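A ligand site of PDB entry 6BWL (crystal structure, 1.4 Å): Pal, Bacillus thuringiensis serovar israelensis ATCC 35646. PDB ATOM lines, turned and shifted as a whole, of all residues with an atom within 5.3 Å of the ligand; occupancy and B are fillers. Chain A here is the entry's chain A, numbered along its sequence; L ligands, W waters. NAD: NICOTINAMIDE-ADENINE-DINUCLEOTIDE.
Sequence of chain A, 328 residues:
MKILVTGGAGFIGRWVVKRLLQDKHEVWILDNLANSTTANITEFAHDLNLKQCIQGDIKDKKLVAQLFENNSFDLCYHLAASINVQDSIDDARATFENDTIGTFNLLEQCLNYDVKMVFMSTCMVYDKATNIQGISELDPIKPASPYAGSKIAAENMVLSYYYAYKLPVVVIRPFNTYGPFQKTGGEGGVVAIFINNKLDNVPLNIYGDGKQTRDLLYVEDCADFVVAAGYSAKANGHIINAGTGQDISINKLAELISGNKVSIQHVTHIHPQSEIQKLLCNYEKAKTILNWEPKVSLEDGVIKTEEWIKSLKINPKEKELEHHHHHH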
ATOM      1  N   GLY A   7     -21.446  -1.272  23.731  1.00  0.00           N
ATOM      2  CA  GLY A   7     -20.885  -0.362  22.761  1.00  0.00           C
ATOM      3  C   GLY A   7     -19.452   0.025  23.050  1.00  0.00           C
ATOM      4  O   GLY A   7     -18.936   1.011  22.505  1.00  0.00           O
ATOM      5  N   ALA A   9     -16.629  -1.108  22.069  1.00  0.00           N
ATOM      6  CA  ALA A   9     -15.651  -1.065  20.972  1.00  0.00           C
ATOM      7  C   ALA A   9     -15.865   0.126  20.057  1.00  0.00           C
ATOM      8  O   ALA A   9     -15.115   0.274  19.104  1.00  0.00           O
ATOM      9  CB  ALA A   9     -15.732  -2.339  20.151  1.00  0.00           C
ATOM     10  N   GLY A  10     -16.854   0.951  20.366  1.00  0.00           N
ATOM     11  CA  GLY A  10     -17.105   2.128  19.544  1.00  0.00           C
ATOM     12  C   GLY A  10     -16.219   3.317  19.900  1.00  0.00           C
ATOM     13  O   GLY A  10     -15.247   3.222  20.641  1.00  0.00           O
ATOM     14  N   PHE A  11     -16.560   4.441  19.276  1.00  0.00           N
ATOM     15  CA  PHE A  11     -15.775   5.667  19.384  1.00  0.00           C
ATOM     16  C   PHE A  11     -15.673   6.194  20.812  1.00  0.00           C
ATOM     17  O   PHE A  11     -14.600   6.249  21.412  1.00  0.00           O
ATOM     18  CB  PHE A  11     -16.377   6.693  18.415  1.00  0.00           C
ATOM     19  CG  PHE A  11     -16.041   8.134  18.709  1.00  0.00           C
ATOM     20  CD1 PHE A  11     -17.055   9.086  18.704  1.00  0.00           C
ATOM     21  CD2 PHE A  11     -14.740   8.563  18.967  1.00  0.00           C
ATOM     22  CE1 PHE A  11     -16.786  10.405  18.978  1.00  0.00           C
ATOM     23  CE2 PHE A  11     -14.462   9.896  19.234  1.00  0.00           C
ATOM     24  CZ  PHE A  11     -15.494  10.803  19.235  1.00  0.00           C
ATOM     25  N   ILE A  12     -16.810   6.554  21.394  1.00  0.00           N
ATOM     26  CA  ILE A  12     -16.789   7.027  22.764  1.00  0.00           C
ATOM     27  C   ILE A  12     -16.515   5.878  23.713  1.00  0.00           C
ATOM     28  O   ILE A  12     -15.749   5.982  24.687  1.00  0.00           O
ATOM     29  CB  ILE A  12     -18.073   7.763  23.162  1.00  0.00           C
ATOM     30  CG1 ILE A  12     -18.338   8.944  22.214  1.00  0.00           C
ATOM     31  CG2 ILE A  12     -17.988   8.203  24.623  1.00  0.00           C
ATOM     32  CD1 ILE A  12     -19.649   9.642  22.396  1.00  0.00           C
ATOM     33  N   GLY A  13     -17.089   4.716  23.406  1.00  0.00           N
ATOM     34  CA  GLY A  13     -16.938   3.509  24.222  1.00  0.00           C
ATOM     35  C   GLY A  13     -15.527   3.095  24.482  1.00  0.00           C
ATOM     36  O   GLY A  13     -15.175   2.742  25.616  1.00  0.00           O
ATOM     37  N   LEU A  30     -19.724  -5.480  25.517  1.00  0.00           N
ATOM     38  CA  LEU A  30     -20.702  -6.126  24.673  1.00  0.00           C
ATOM     39  C   LEU A  30     -20.901  -5.234  23.443  1.00  0.00           C
ATOM     40  O   LEU A  30     -21.334  -4.078  23.593  1.00  0.00           O
ATOM     41  CB  LEU A  30     -22.031  -6.329  25.386  1.00  0.00           C
ATOM     42  CG  LEU A  30     -23.162  -6.867  24.536  1.00  0.00           C
ATOM     43  CD1 LEU A  30     -22.858  -8.270  24.012  1.00  0.00           C
ATOM     44  CD2 LEU A  30     -24.472  -6.914  25.317  1.00  0.00           C
ATOM     45  N   ASP A  31     -20.555  -5.705  22.249  1.00  0.00           N
ATOM     46  CA  ASP A  31     -20.591  -4.871  21.065  1.00  0.00           C
ATOM     47  C   ASP A  31     -20.776  -5.783  19.839  1.00  0.00           C
ATOM     48  O   ASP A  31     -20.027  -6.734  19.718  1.00  0.00           O
ATOM     49  CB  ASP A  31     -19.323  -4.020  20.990  1.00  0.00           C
ATOM     50  CG  ASP A  31     -19.458  -2.848  20.042  1.00  0.00           C
ATOM     51  OD1 ASP A  31     -19.829  -3.023  18.864  1.00  0.00           O
ATOM     52  OD2 ASP A  31     -19.168  -1.693  20.500  1.00  0.00           O
ATOM     53  N   ASN A  32     -21.718  -5.472  18.974  1.00  0.00           N
ATOM     54  CA  ASN A  32     -21.981  -6.344  17.810  1.00  0.00           C
ATOM     55  C   ASN A  32     -21.075  -5.917  16.655  1.00  0.00           C
ATOM     56  O   ASN A  32     -21.162  -6.509  15.575  1.00  0.00           O
ATOM     57  CB  ASN A  32     -23.459  -6.313  17.400  1.00  0.00           C
ATOM     58  CG  ASN A  32     -23.951  -4.963  16.910  1.00  0.00           C
ATOM     59  OD1 ASN A  32     -23.225  -3.977  16.888  1.00  0.00           O
ATOM     60  ND2 ASN A  32     -25.250  -4.900  16.503  1.00  0.00           N
ATOM     61  N   LEU A  33     -20.242  -4.894  16.824  1.00  0.00           N
ATOM     62  CA  LEU A  33     -19.343  -4.405  15.788  1.00  0.00           C
ATOM     63  C   LEU A  33     -20.093  -3.949  14.541  1.00  0.00           C
ATOM     64  O   LEU A  33     -19.505  -3.917  13.436  1.00  0.00           O
ATOM     65  CB  LEU A  33     -18.228  -5.445  15.488  1.00  0.00           C
ATOM     66  CG  LEU A  33     -17.373  -5.829  16.661  1.00  0.00           C
ATOM     67  CD1 LEU A  33     -16.305  -6.847  16.212  1.00  0.00           C
ATOM     68  CD2 LEU A  33     -16.687  -4.644  17.282  1.00  0.00           C
ATOM     69  N   ALA A  34     -21.329  -3.501  14.680  1.00  0.00           N
ATOM     70  CA  ALA A  34     -22.075  -3.028  13.556  1.00  0.00           C
ATOM     71  C   ALA A  34     -21.516  -1.709  13.036  1.00  0.00           C
ATOM     72  O   ALA A  34     -21.639  -1.419  11.847  1.00  0.00           O
ATOM     73  CB  ALA A  34     -23.537  -2.879  13.894  1.00  0.00           C
ATOM     74  N   ASN A  35     -20.912  -0.905  13.903  1.00  0.00           N
ATOM     75  CA  ASN A  35     -20.398   0.408  13.512  1.00  0.00           C
ATOM     76  C   ASN A  35     -18.955   0.617  13.937  1.00  0.00           C
ATOM     77  O   ASN A  35     -18.480   1.743  13.990  1.00  0.00           O
ATOM     78  CB  ASN A  35     -21.237   1.590  14.043  1.00  0.00           C
ATOM     79  CG  ASN A  35     -20.937   2.935  13.299  1.00  0.00           C
ATOM     80  OD1 ASN A  35     -20.745   2.916  12.034  1.00  0.00           O
ATOM     81  ND2 ASN A  35     -20.909   4.115  14.002  1.00  0.00           N
ATOM     82  N   SER A  36     -18.228  -0.464  14.196  1.00  0.00           N
ATOM     83  CA  SER A  36     -16.861  -0.354  14.684  1.00  0.00           C
ATOM     84  C   SER A  36     -16.073  -1.584  14.341  1.00  0.00           C
ATOM     85  O   SER A  36     -16.660  -2.543  13.832  1.00  0.00           O
ATOM     86  CB  SER A  36     -16.888  -0.141  16.206  1.00  0.00           C
ATOM     87  OG  SER A  36     -17.507  -1.231  16.856  1.00  0.00           O
ATOM     88  N   GLY A  56     -21.945  -9.569  20.381  1.00  0.00           N
ATOM     89  CA  GLY A  56     -23.319  -9.990  20.557  1.00  0.00           C
ATOM     90  C   GLY A  56     -24.192  -8.740  20.528  1.00  0.00           C
ATOM     91  O   GLY A  56     -23.697  -7.625  20.555  1.00  0.00           O
ATOM     92  N   ASP A  57     -25.480  -8.982  20.456  1.00  0.00           N
ATOM     93  CA  ASP A  57     -26.458  -7.943  20.130  1.00  0.00           C
ATOM     94  C   ASP A  57     -27.349  -7.712  21.325  1.00  0.00           C
ATOM     95  O   ASP A  57     -27.905  -8.652  21.889  1.00  0.00           O
ATOM     96  CB  ASP A  57     -27.295  -8.358  18.927  1.00  0.00           C
ATOM     97  CG  ASP A  57     -27.872  -7.141  18.220  1.00  0.00           C
ATOM     98  OD1 ASP A  57     -28.657  -6.442  18.815  1.00  0.00           O
ATOM     99  OD2 ASP A  57     -27.423  -6.805  17.096  1.00  0.00           O
ATOM    100  N   ILE A  58     -27.494  -6.454  21.724  1.00  0.00           N
ATOM    101  CA  ILE A  58     -28.412  -6.100  22.816  1.00  0.00           C
ATOM    102  C   ILE A  58     -29.888  -6.424  22.499  1.00  0.00           C
ATOM    103  O   ILE A  58     -30.713  -6.448  23.405  1.00  0.00           O
ATOM    104  CB  ILE A  58     -28.280  -4.619  23.284  1.00  0.00           C
ATOM    105  CG1 ILE A  58     -28.726  -3.664  22.165  1.00  0.00           C
ATOM    106  CG2 ILE A  58     -26.849  -4.353  23.699  1.00  0.00           C
ATOM    107  CD1 ILE A  58     -28.706  -2.208  22.554  1.00  0.00           C
ATOM    108  N   LYS A  59     -30.212  -6.635  21.219  1.00  0.00           N
ATOM    109  CA  LYS A  59     -31.547  -7.074  20.842  1.00  0.00           C
ATOM    110  C   LYS A  59     -31.783  -8.555  21.063  1.00  0.00           C
ATOM    111  O   LYS A  59     -32.898  -9.007  20.958  1.00  0.00           O
ATOM    112  CB  LYS A  59     -31.871  -6.750  19.387  1.00  0.00           C
ATOM    113  CG  LYS A  59     -31.759  -5.256  19.071  1.00  0.00           C
ATOM    114  CD  LYS A  59     -32.241  -4.950  17.659  1.00  0.00           C
ATOM    115  CE  LYS A  59     -31.445  -5.642  16.586  1.00  0.00           C
ATOM    116  NZ  LYS A  59     -30.032  -5.293  16.573  1.00  0.00           N
ATOM    117  N   HIS A  78     -24.265   2.001  29.294  1.00  0.00           N
ATOM    118  CA  HIS A  78     -25.010   1.565  28.122  1.00  0.00           C
ATOM    119  C   HIS A  78     -24.868   2.553  26.987  1.00  0.00           C
ATOM    120  O   HIS A  78     -25.636   3.533  26.884  1.00  0.00           O
ATOM    121  CB  HIS A  78     -26.460   1.272  28.498  1.00  0.00           C
ATOM    122  CG  HIS A  78     -27.288   0.917  27.306  1.00  0.00           C
ATOM    123  ND1 HIS A  78     -26.752   0.218  26.243  1.00  0.00           N
ATOM    124  CD2 HIS A  78     -28.551   1.239  26.952  1.00  0.00           C
ATOM    125  CE1 HIS A  78     -27.657   0.129  25.281  1.00  0.00           C
ATOM    126  NE2 HIS A  78     -28.767   0.732  25.696  1.00  0.00           N
ATOM    127  N   LEU A  79     -23.843   2.314  26.134  1.00  0.00           N
ATOM    128  CA  LEU A  79     -23.518   3.152  24.978  1.00  0.00           C
ATOM    129  C   LEU A  79     -23.934   2.560  23.657  1.00  0.00           C
ATOM    130  O   LEU A  79     -23.940   3.265  22.648  1.00  0.00           O
ATOM    131  CB  LEU A  79     -22.035   3.531  24.973  1.00  0.00           C
ATOM    132  CG  LEU A  79     -21.670   4.740  25.863  1.00  0.00           C
ATOM    133  CD1 LEU A  79     -21.846   4.437  27.339  1.00  0.00           C
ATOM    134  CD2 LEU A  79     -20.238   5.164  25.622  1.00  0.00           C
ATOM    135  N   ALA A  80     -24.195   1.252  23.612  1.00  0.00           N
ATOM    136  CA  ALA A  80     -24.549   0.645  22.336  1.00  0.00           C
ATOM    137  C   ALA A  80     -25.817   1.249  21.766  1.00  0.00           C
ATOM    138  O   ALA A  80     -26.813   1.282  22.455  1.00  0.00           O
ATOM    139  CB  ALA A  80     -24.747  -0.841  22.510  1.00  0.00           C
ATOM    140  N   ALA A  81     -25.785   1.628  20.485  1.00  0.00           N
ATOM    141  CA  ALA A  81     -26.937   2.245  19.829  1.00  0.00           C
ATOM    142  C   ALA A  81     -26.646   2.390  18.353  1.00  0.00           C
ATOM    143  O   ALA A  81     -25.472   2.471  17.964  1.00  0.00           O
ATOM    144  CB  ALA A  81     -27.148   3.638  20.408  1.00  0.00           C
ATOM    145  N   SER A  82     -27.720   2.499  17.569  1.00  0.00           N
ATOM    146  CA  SER A  82     -27.706   3.164  16.267  1.00  0.00           C
ATOM    147  C   SER A  82     -27.675   4.667  16.470  1.00  0.00           C
ATOM    148  O   SER A  82     -28.426   5.186  17.296  1.00  0.00           O
ATOM    149  CB  SER A  82     -28.979   2.800  15.488  1.00  0.00           C
ATOM    150  OG  SER A  82     -29.074   1.404  15.252  1.00  0.00           O
ATOM    151  N   ILE A  83     -26.809   5.389  15.757  1.00  0.00           N
ATOM    152  CA  ILE A  83     -26.520   6.777  16.076  1.00  0.00           C
ATOM    153  C   ILE A  83     -26.786   7.746  14.953  1.00  0.00           C
ATOM    154  O   ILE A  83     -26.598   8.946  15.144  1.00  0.00           O
ATOM    155  CB  ILE A  83     -25.054   6.952  16.563  1.00  0.00           C
ATOM    156  CG1 ILE A  83     -24.069   6.674  15.442  1.00  0.00           C
ATOM    157  CG2 ILE A  83     -24.775   6.023  17.753  1.00  0.00           C
ATOM    158  CD1 ILE A  83     -22.651   7.186  15.682  1.00  0.00           C
ATOM    159  N   ASN A  98     -32.932  -1.001  18.066  1.00  0.00           N
ATOM    160  CA  ASN A  98     -31.617  -0.933  18.723  1.00  0.00           C
ATOM    161  C   ASN A  98     -31.633  -0.009  19.942  1.00  0.00           C
ATOM    162  O   ASN A  98     -30.966  -0.322  20.947  1.00  0.00           O
ATOM    163  CB  ASN A  98     -30.545  -0.479  17.730  1.00  0.00           C
ATOM    164  CG  ASN A  98     -30.143  -1.613  16.800  1.00  0.00           C
ATOM    165  OD1 ASN A  98     -29.592  -2.599  17.231  1.00  0.00           O
ATOM    166  ND2 ASN A  98     -30.514  -1.522  15.538  1.00  0.00           N
ATOM    167  N   MET A 120     -26.637   6.305  28.098  1.00  0.00           N
ATOM    168  CA  MET A 120     -26.136   7.294  27.170  1.00  0.00           C
ATOM    169  C   MET A 120     -27.225   7.803  26.258  1.00  0.00           C
ATOM    170  O   MET A 120     -27.577   7.154  25.265  1.00  0.00           O
ATOM    171  CB  MET A 120     -24.993   6.715  26.346  1.00  0.00           C
ATOM    172  CG  MET A 120     -24.186   7.743  25.579  1.00  0.00           C
ATOM    173  SD  MET A 120     -22.944   8.556  26.643  1.00  0.00           S
ATOM    174  CE  MET A 120     -21.771   9.070  25.433  1.00  0.00           C
ATOM    175  N   SER A 121     -27.751   8.967  26.586  1.00  0.00           N
ATOM    176  CA  SER A 121     -28.682   9.671  25.727  1.00  0.00           C
ATOM    177  C   SER A 121     -27.896  10.681  24.922  1.00  0.00           C
ATOM    178  O   SER A 121     -26.730  10.426  24.634  1.00  0.00           O
ATOM    179  CB  SER A 121     -29.817  10.288  26.533  1.00  0.00           C
ATOM    180  OG  SER A 121     -30.824  10.764  25.625  1.00  0.00           O
ATOM    181  N   THR A 122     -28.510  11.777  24.482  1.00  0.00           N
ATOM    182  CA  THR A 122     -27.919  12.623  23.454  1.00  0.00           C
ATOM    183  C   THR A 122     -28.530  14.030  23.556  1.00  0.00           C
ATOM    184  O   THR A 122     -29.702  14.168  23.898  1.00  0.00           O
ATOM    185  CB  THR A 122     -28.149  12.057  22.071  1.00  0.00           C
ATOM    186  OG1 THR A 122     -27.720  13.058  21.108  1.00  0.00           O
ATOM    187  CG2 THR A 122     -29.583  11.739  21.796  1.00  0.00           C
ATOM    188  N   CYS A 123     -27.736  15.049  23.245  1.00  0.00           N
ATOM    189  CA  CYS A 123     -28.208  16.432  23.300  1.00  0.00           C
ATOM    190  C   CYS A 123     -29.160  16.731  22.153  1.00  0.00           C
ATOM    191  O   CYS A 123     -29.672  17.846  22.036  1.00  0.00           O
ATOM    192  CB  CYS A 123     -27.021  17.394  23.269  1.00  0.00           C
ATOM    193  SG  CYS A 123     -26.226  17.543  21.653  1.00  0.00           S
ATOM    194  N   TYR A 147     -34.355   8.807  15.598  1.00  0.00           N
ATOM    195  CA  TYR A 147     -33.234   8.662  16.538  1.00  0.00           C
ATOM    196  C   TYR A 147     -33.512   9.399  17.849  1.00  0.00           C
ATOM    197  O   TYR A 147     -33.406   8.805  18.937  1.00  0.00           O
ATOM    198  CB  TYR A 147     -31.929   9.166  15.905  1.00  0.00           C
ATOM    199  CG  TYR A 147     -30.765   9.274  16.850  1.00  0.00           C
ATOM    200  CD1 TYR A 147     -30.223  10.505  17.142  1.00  0.00           C
ATOM    201  CD2 TYR A 147     -30.176   8.149  17.398  1.00  0.00           C
ATOM    202  CE1 TYR A 147     -29.131  10.605  17.992  1.00  0.00           C
ATOM    203  CE2 TYR A 147     -29.095   8.215  18.226  1.00  0.00           C
ATOM    204  CZ  TYR A 147     -28.583   9.454  18.522  1.00  0.00           C
ATOM    205  OH  TYR A 147     -27.473   9.585  19.350  1.00  0.00           O
ATOM    206  N   LYS A 151     -34.289   7.713  21.595  1.00  0.00           N
ATOM    207  CA  LYS A 151     -33.460   8.022  22.770  1.00  0.00           C
ATOM    208  C   LYS A 151     -34.310   8.546  23.922  1.00  0.00           C
ATOM    209  O   LYS A 151     -34.126   8.125  25.060  1.00  0.00           O
ATOM    210  CB  LYS A 151     -32.337   9.000  22.406  1.00  0.00           C
ATOM    211  CG  LYS A 151     -31.219   8.321  21.621  1.00  0.00           C
ATOM    212  CD  LYS A 151     -30.363   7.409  22.492  1.00  0.00           C
ATOM    213  CE  LYS A 151     -29.036   7.027  21.861  1.00  0.00           C
ATOM    214  NZ  LYS A 151     -28.201   6.169  22.731  1.00  0.00           N
ATOM    215  N   PRO A 174     -24.775  13.987  26.704  1.00  0.00           N
ATOM    216  CA  PRO A 174     -23.632  14.697  26.144  1.00  0.00           C
ATOM    217  C   PRO A 174     -23.988  15.312  24.820  1.00  0.00           C
ATOM    218  O   PRO A 174     -24.816  14.800  24.050  1.00  0.00           O
ATOM    219  CB  PRO A 174     -22.560  13.618  26.003  1.00  0.00           C
ATOM    220  CG  PRO A 174     -23.197  12.330  26.325  1.00  0.00           C
ATOM    221  CD  PRO A 174     -24.643  12.528  26.616  1.00  0.00           C
ATOM    222  N   PHE A 175     -23.315  16.430  24.530  1.00  0.00           N
ATOM    223  CA  PHE A 175     -23.451  17.106  23.250  1.00  0.00           C
ATOM    224  C   PHE A 175     -22.464  16.495  22.250  1.00  0.00           C
ATOM    225  O   PHE A 175     -21.618  15.653  22.614  1.00  0.00           O
ATOM    226  CB  PHE A 175     -23.309  18.618  23.462  1.00  0.00           C
ATOM    227  CG  PHE A 175     -24.566  19.283  23.992  1.00  0.00           C
ATOM    228  CD1 PHE A 175     -25.219  20.259  23.242  1.00  0.00           C
ATOM    229  CD2 PHE A 175     -25.151  18.903  25.202  1.00  0.00           C
ATOM    230  CE1 PHE A 175     -26.377  20.878  23.729  1.00  0.00           C
ATOM    231  CE2 PHE A 175     -26.328  19.446  25.662  1.00  0.00           C
ATOM    232  CZ  PHE A 175     -26.952  20.473  24.919  1.00  0.00           C
ATOM    233  N   ASN A 176     -22.601  16.866  20.986  1.00  0.00           N
ATOM    234  CA  ASN A 176     -21.829  16.310  19.889  1.00  0.00           C
ATOM    235  C   ASN A 176     -20.369  16.156  20.286  1.00  0.00           C
ATOM    236  O   ASN A 176     -19.736  17.113  20.685  1.00  0.00           O
ATOM    237  CB  ASN A 176     -21.899  17.237  18.656  1.00  0.00           C
ATOM    238  CG  ASN A 176     -23.265  17.308  18.053  1.00  0.00           C
ATOM    239  OD1 ASN A 176     -24.201  17.739  18.705  1.00  0.00           O
ATOM    240  ND2 ASN A 176     -23.392  16.863  16.805  1.00  0.00           N
ATOM    241  N   THR A 177     -19.855  14.939  20.131  1.00  0.00           N
ATOM    242  CA  THR A 177     -18.537  14.574  20.574  1.00  0.00           C
ATOM    243  C   THR A 177     -17.654  14.227  19.378  1.00  0.00           C
ATOM    244  O   THR A 177     -18.147  13.625  18.399  1.00  0.00           O
ATOM    245  CB  THR A 177     -18.662  13.399  21.553  1.00  0.00           C
ATOM    246  OG1 THR A 177     -19.409  13.831  22.698  1.00  0.00           O
ATOM    247  CG2 THR A 177     -17.340  12.894  22.029  1.00  0.00           C
ATOM    248  N   GLN A 182     -13.155   8.346  16.057  1.00  0.00           N
ATOM    249  CA  GLN A 182     -14.388   8.567  15.343  1.00  0.00           C
ATOM    250  C   GLN A 182     -14.180   8.331  13.858  1.00  0.00           C
ATOM    251  O   GLN A 182     -13.212   8.803  13.272  1.00  0.00           O
ATOM    252  CB  GLN A 182     -14.894   9.975  15.590  1.00  0.00           C
ATOM    253  CG  GLN A 182     -16.265  10.227  14.959  1.00  0.00           C
ATOM    254  CD  GLN A 182     -16.873  11.552  15.339  1.00  0.00           C
ATOM    255  OE1 GLN A 182     -16.274  12.609  15.180  1.00  0.00           O
ATOM    256  NE2 GLN A 182     -18.074  11.516  15.863  1.00  0.00           N
HETATM  257  PA  NAD L   1     -20.395   4.234  17.833  1.00  0.00           P
HETATM  258  O1A NAD L   1     -21.244   3.697  16.756  1.00  0.00           O
HETATM  259  O2A NAD L   1     -18.922   4.296  17.648  1.00  0.00           O
HETATM  260  O5B NAD L   1     -20.632   3.429  19.222  1.00  0.00           O
HETATM  261  C5B NAD L   1     -21.766   2.583  19.400  1.00  0.00           C
HETATM  262  C4B NAD L   1     -21.238   1.159  19.487  1.00  0.00           C
HETATM  263  O4B NAD L   1     -22.389   0.320  19.733  1.00  0.00           O
HETATM  264  C3B NAD L   1     -20.552   0.600  18.223  1.00  0.00           C
HETATM  265  O3B NAD L   1     -19.276   0.046  18.513  1.00  0.00           O
HETATM  266  C2B NAD L   1     -21.590  -0.374  17.687  1.00  0.00           C
HETATM  267  O2B NAD L   1     -20.994  -1.417  16.920  1.00  0.00           O
HETATM  268  C1B NAD L   1     -22.291  -0.891  18.917  1.00  0.00           C
HETATM  269  N9A NAD L   1     -23.661  -1.304  18.700  1.00  0.00           N
HETATM  270  C8A NAD L   1     -24.625  -0.715  17.950  1.00  0.00           C
HETATM  271  N7A NAD L   1     -25.799  -1.361  17.990  1.00  0.00           N
HETATM  272  C5A NAD L   1     -25.571  -2.421  18.814  1.00  0.00           C
HETATM  273  C6A NAD L   1     -26.359  -3.561  19.219  1.00  0.00           C
HETATM  274  N6A NAD L   1     -27.641  -3.720  18.837  1.00  0.00           N
HETATM  275  N1A NAD L   1     -25.775  -4.434  20.064  1.00  0.00           N
HETATM  276  C2A NAD L   1     -24.482  -4.322  20.428  1.00  0.00           C
HETATM  277  N3A NAD L   1     -23.649  -3.322  20.087  1.00  0.00           N
HETATM  278  C4A NAD L   1     -24.193  -2.396  19.271  1.00  0.00           C
HETATM  279  O3  NAD L   1     -20.906   5.706  18.221  1.00  0.00           O
HETATM  280  PN  NAD L   1     -20.458   6.762  19.328  1.00  0.00           P
HETATM  281  O1N NAD L   1     -20.386   8.081  18.650  1.00  0.00           O
HETATM  282  O2N NAD L   1     -19.324   6.211  20.095  1.00  0.00           O
HETATM  283  O5D NAD L   1     -21.775   6.779  20.251  1.00  0.00           O
HETATM  284  C5D NAD L   1     -21.820   6.004  21.449  1.00  0.00           C
HETATM  285  C4D NAD L   1     -23.060   6.382  22.235  1.00  0.00           C
HETATM  286  O4D NAD L   1     -23.023   7.803  22.547  1.00  0.00           O
HETATM  287  C3D NAD L   1     -24.366   6.182  21.476  1.00  0.00           C
HETATM  288  O3D NAD L   1     -25.391   5.731  22.403  1.00  0.00           O
HETATM  289  C2D NAD L   1     -24.758   7.553  20.988  1.00  0.00           C
HETATM  290  O2D NAD L   1     -26.170   7.673  20.801  1.00  0.00           O
HETATM  291  C1D NAD L   1     -24.237   8.452  22.087  1.00  0.00           C
HETATM  292  N1N NAD L   1     -23.873   9.820  21.744  1.00  0.00           N
HETATM  293  C2N NAD L   1     -22.946  10.077  20.760  1.00  0.00           C
HETATM  294  C3N NAD L   1     -22.567  11.370  20.506  1.00  0.00           C
HETATM  295  C7N NAD L   1     -21.636  11.701  19.410  1.00  0.00           C
HETATM  296  O7N NAD L   1     -21.549  12.881  19.021  1.00  0.00           O
HETATM  297  N7N NAD L   1     -20.906  10.769  18.806  1.00  0.00           N
HETATM  298  C4N NAD L   1     -23.093  12.436  21.299  1.00  0.00           C
HETATM  299  C5N NAD L   1     -24.017  12.109  22.300  1.00  0.00           C
HETATM  300  C6N NAD L   1     -24.377  10.801  22.537  1.00  0.00           C
HETATM  301  O   HOH W   1     -17.598   3.965  15.413  1.00  0.00           O
HETATM  302  O   HOH W   2     -22.041  11.019  15.718  1.00  0.00           O
HETATM  303  O   HOH W   3     -26.914   3.667  24.187  1.00  0.00           O
HETATM  304  O   HOH W   4     -19.280   3.855  21.846  1.00  0.00           O
HETATM  305  O   HOH W   5     -23.531   2.402  16.075  1.00  0.00           O
HETATM  306  O   HOH W   6     -19.702   9.008  16.196  1.00  0.00           O
HETATM  307  O   HOH W   7     -27.001  -0.458  15.670  1.00  0.00           O
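OD2 of Asp 31 is in hydrogen-bond range of N of Ala 9 (3.0 Å). The side-chain amide nitrogen of Asn 98 sits at hydrogen-bond distance from the side-chain hydroxyl of Ser 82. NE2 of Gln 182 sits at hydrogen-bond distance from O of Thr 177 (3.3 Å). The side-chain carboxylate (OD2) of Asp 57 lies within hydrogen-bond range of the side-chain amide nitrogen (ND2) of Asn 32 (3.0 Å). OD1 of Asp 57 lies within salt-bridge range of NZ of Lys 59. OD1 of Asn 32 lies within hydrogen-bond range of N of Ala 34 (2.9 Å). The backbone NH of Asn 32 is in hydrogen-bond range of the backbone carbonyl oxygen of Gly 56, at 3.3 Å. The side-chain amide oxygen (OD1) of Asn 176 lies within hydrogen-bond range of the side-chain sulfur (SG) of Cys 123 (3.6 Å).
The side-chain carboxylate (OD2) of Asp 31 is in hydrogen-bond range of an oxygen (O3B) of the ligand (2.6 Å). The side-chain hydroxyl (OH) of Tyr 147 lies within hydrogen-bond range of an oxygen (O2D) of the ligand (2.7 Å). OG of Ser 36 is in hydrogen-bond range of O3B of the ligand, at 2.7 Å. A nitrogen (N6A) of the ligand lies within hydrogen-bond range of the side-chain amide oxygen (OD1) of Asn 98 (2.8 Å). An oxygen (O2B) of the ligand sits at hydrogen-bond distance from the backbone NH of Asn 35 (3.1 Å). The side-chain amide nitrogen of Asn 35 lies within hydrogen-bond range of an oxygen (O1A) of the ligand (2.8 Å). N of Ile 12 lies within hydrogen-bond range of O2N of the ligand. An oxygen (O3D) of the ligand is in hydrogen-bond range of the side-chain amino group (NZ) of Lys 151 (2.9 Å). The backbone carbonyl oxygen (O) of Leu 79 sits at hydrogen-bond distance from an oxygen (O3D) of the ligand. An oxygen (O2A) of the ligand lies within hydrogen-bond range of the backbone NH (N) of Phe 11. O7N of the ligand lies within hydrogen-bond range of N of Thr 177, at 2.9 Å. The side-chain carboxylate of Asp 57 sits at hydrogen-bond distance from a nitrogen (N6A) of the ligand, 2.9 Å away. The backbone NH of Asn 32 sits at hydrogen-bond distance from a nitrogen (N3A) of the ligand, at 3.1 Å. A nitrogen (N3A) of the ligand lies close to the side-chain amide oxygen of Asn 32, at 3.3 Å. N of Ala 34 lies within hydrogen-bond range of O2B of the ligand (3.1 Å). The backbone NH of Ile 58 is in hydrogen-bond range of a nitrogen (N1A) of the ligand. An oxygen (O3B) of the ligand sits close to the backbone NH (N) of Gly 10, 3.2 Å away.
Water W1 bridges O2A of the ligand (2.6 Å) and O of Asn 35 (2.8 Å). Water W6 lies within hydrogen-bond range of an oxygen (O1N) of the ligand (2.7 Å) and the side-chain amide nitrogen of Gln 182 (3.0 Å). Water W5 lies within hydrogen-bond range of O of Ala 81 (2.7 Å) and O1A of the ligand (2.7 Å). Water W7 lies within hydrogen-bond range of N7A of the ligand (2.8 Å) and OG of Ser 82 (2.8 Å). Water W4 lies within hydrogen-bond range of the backbone NH (N) of Gly 13 (2.8 Å), an oxygen (O2N) of the ligand (2.9 Å) and the backbone carbonyl oxygen (O) of Gly 7 (2.9 Å).
Residues that only touch the ligand: Ser 121 (3.2 Å), Met 120 (3.2 Å), Ala 81 (3.3 Å), Pro 174 (3.3 Å), Gly 56 (3.4 Å), Ala 80 (3.4 Å), Ile 83 (3.4 Å), Gly 7 (3.4 Å), Asn 176 (3.5 Å), Leu 33 (3.6 Å), Lys 59 (3.6 Å), Ala 9 (3.7 Å) and Phe 175 (3.8 Å).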
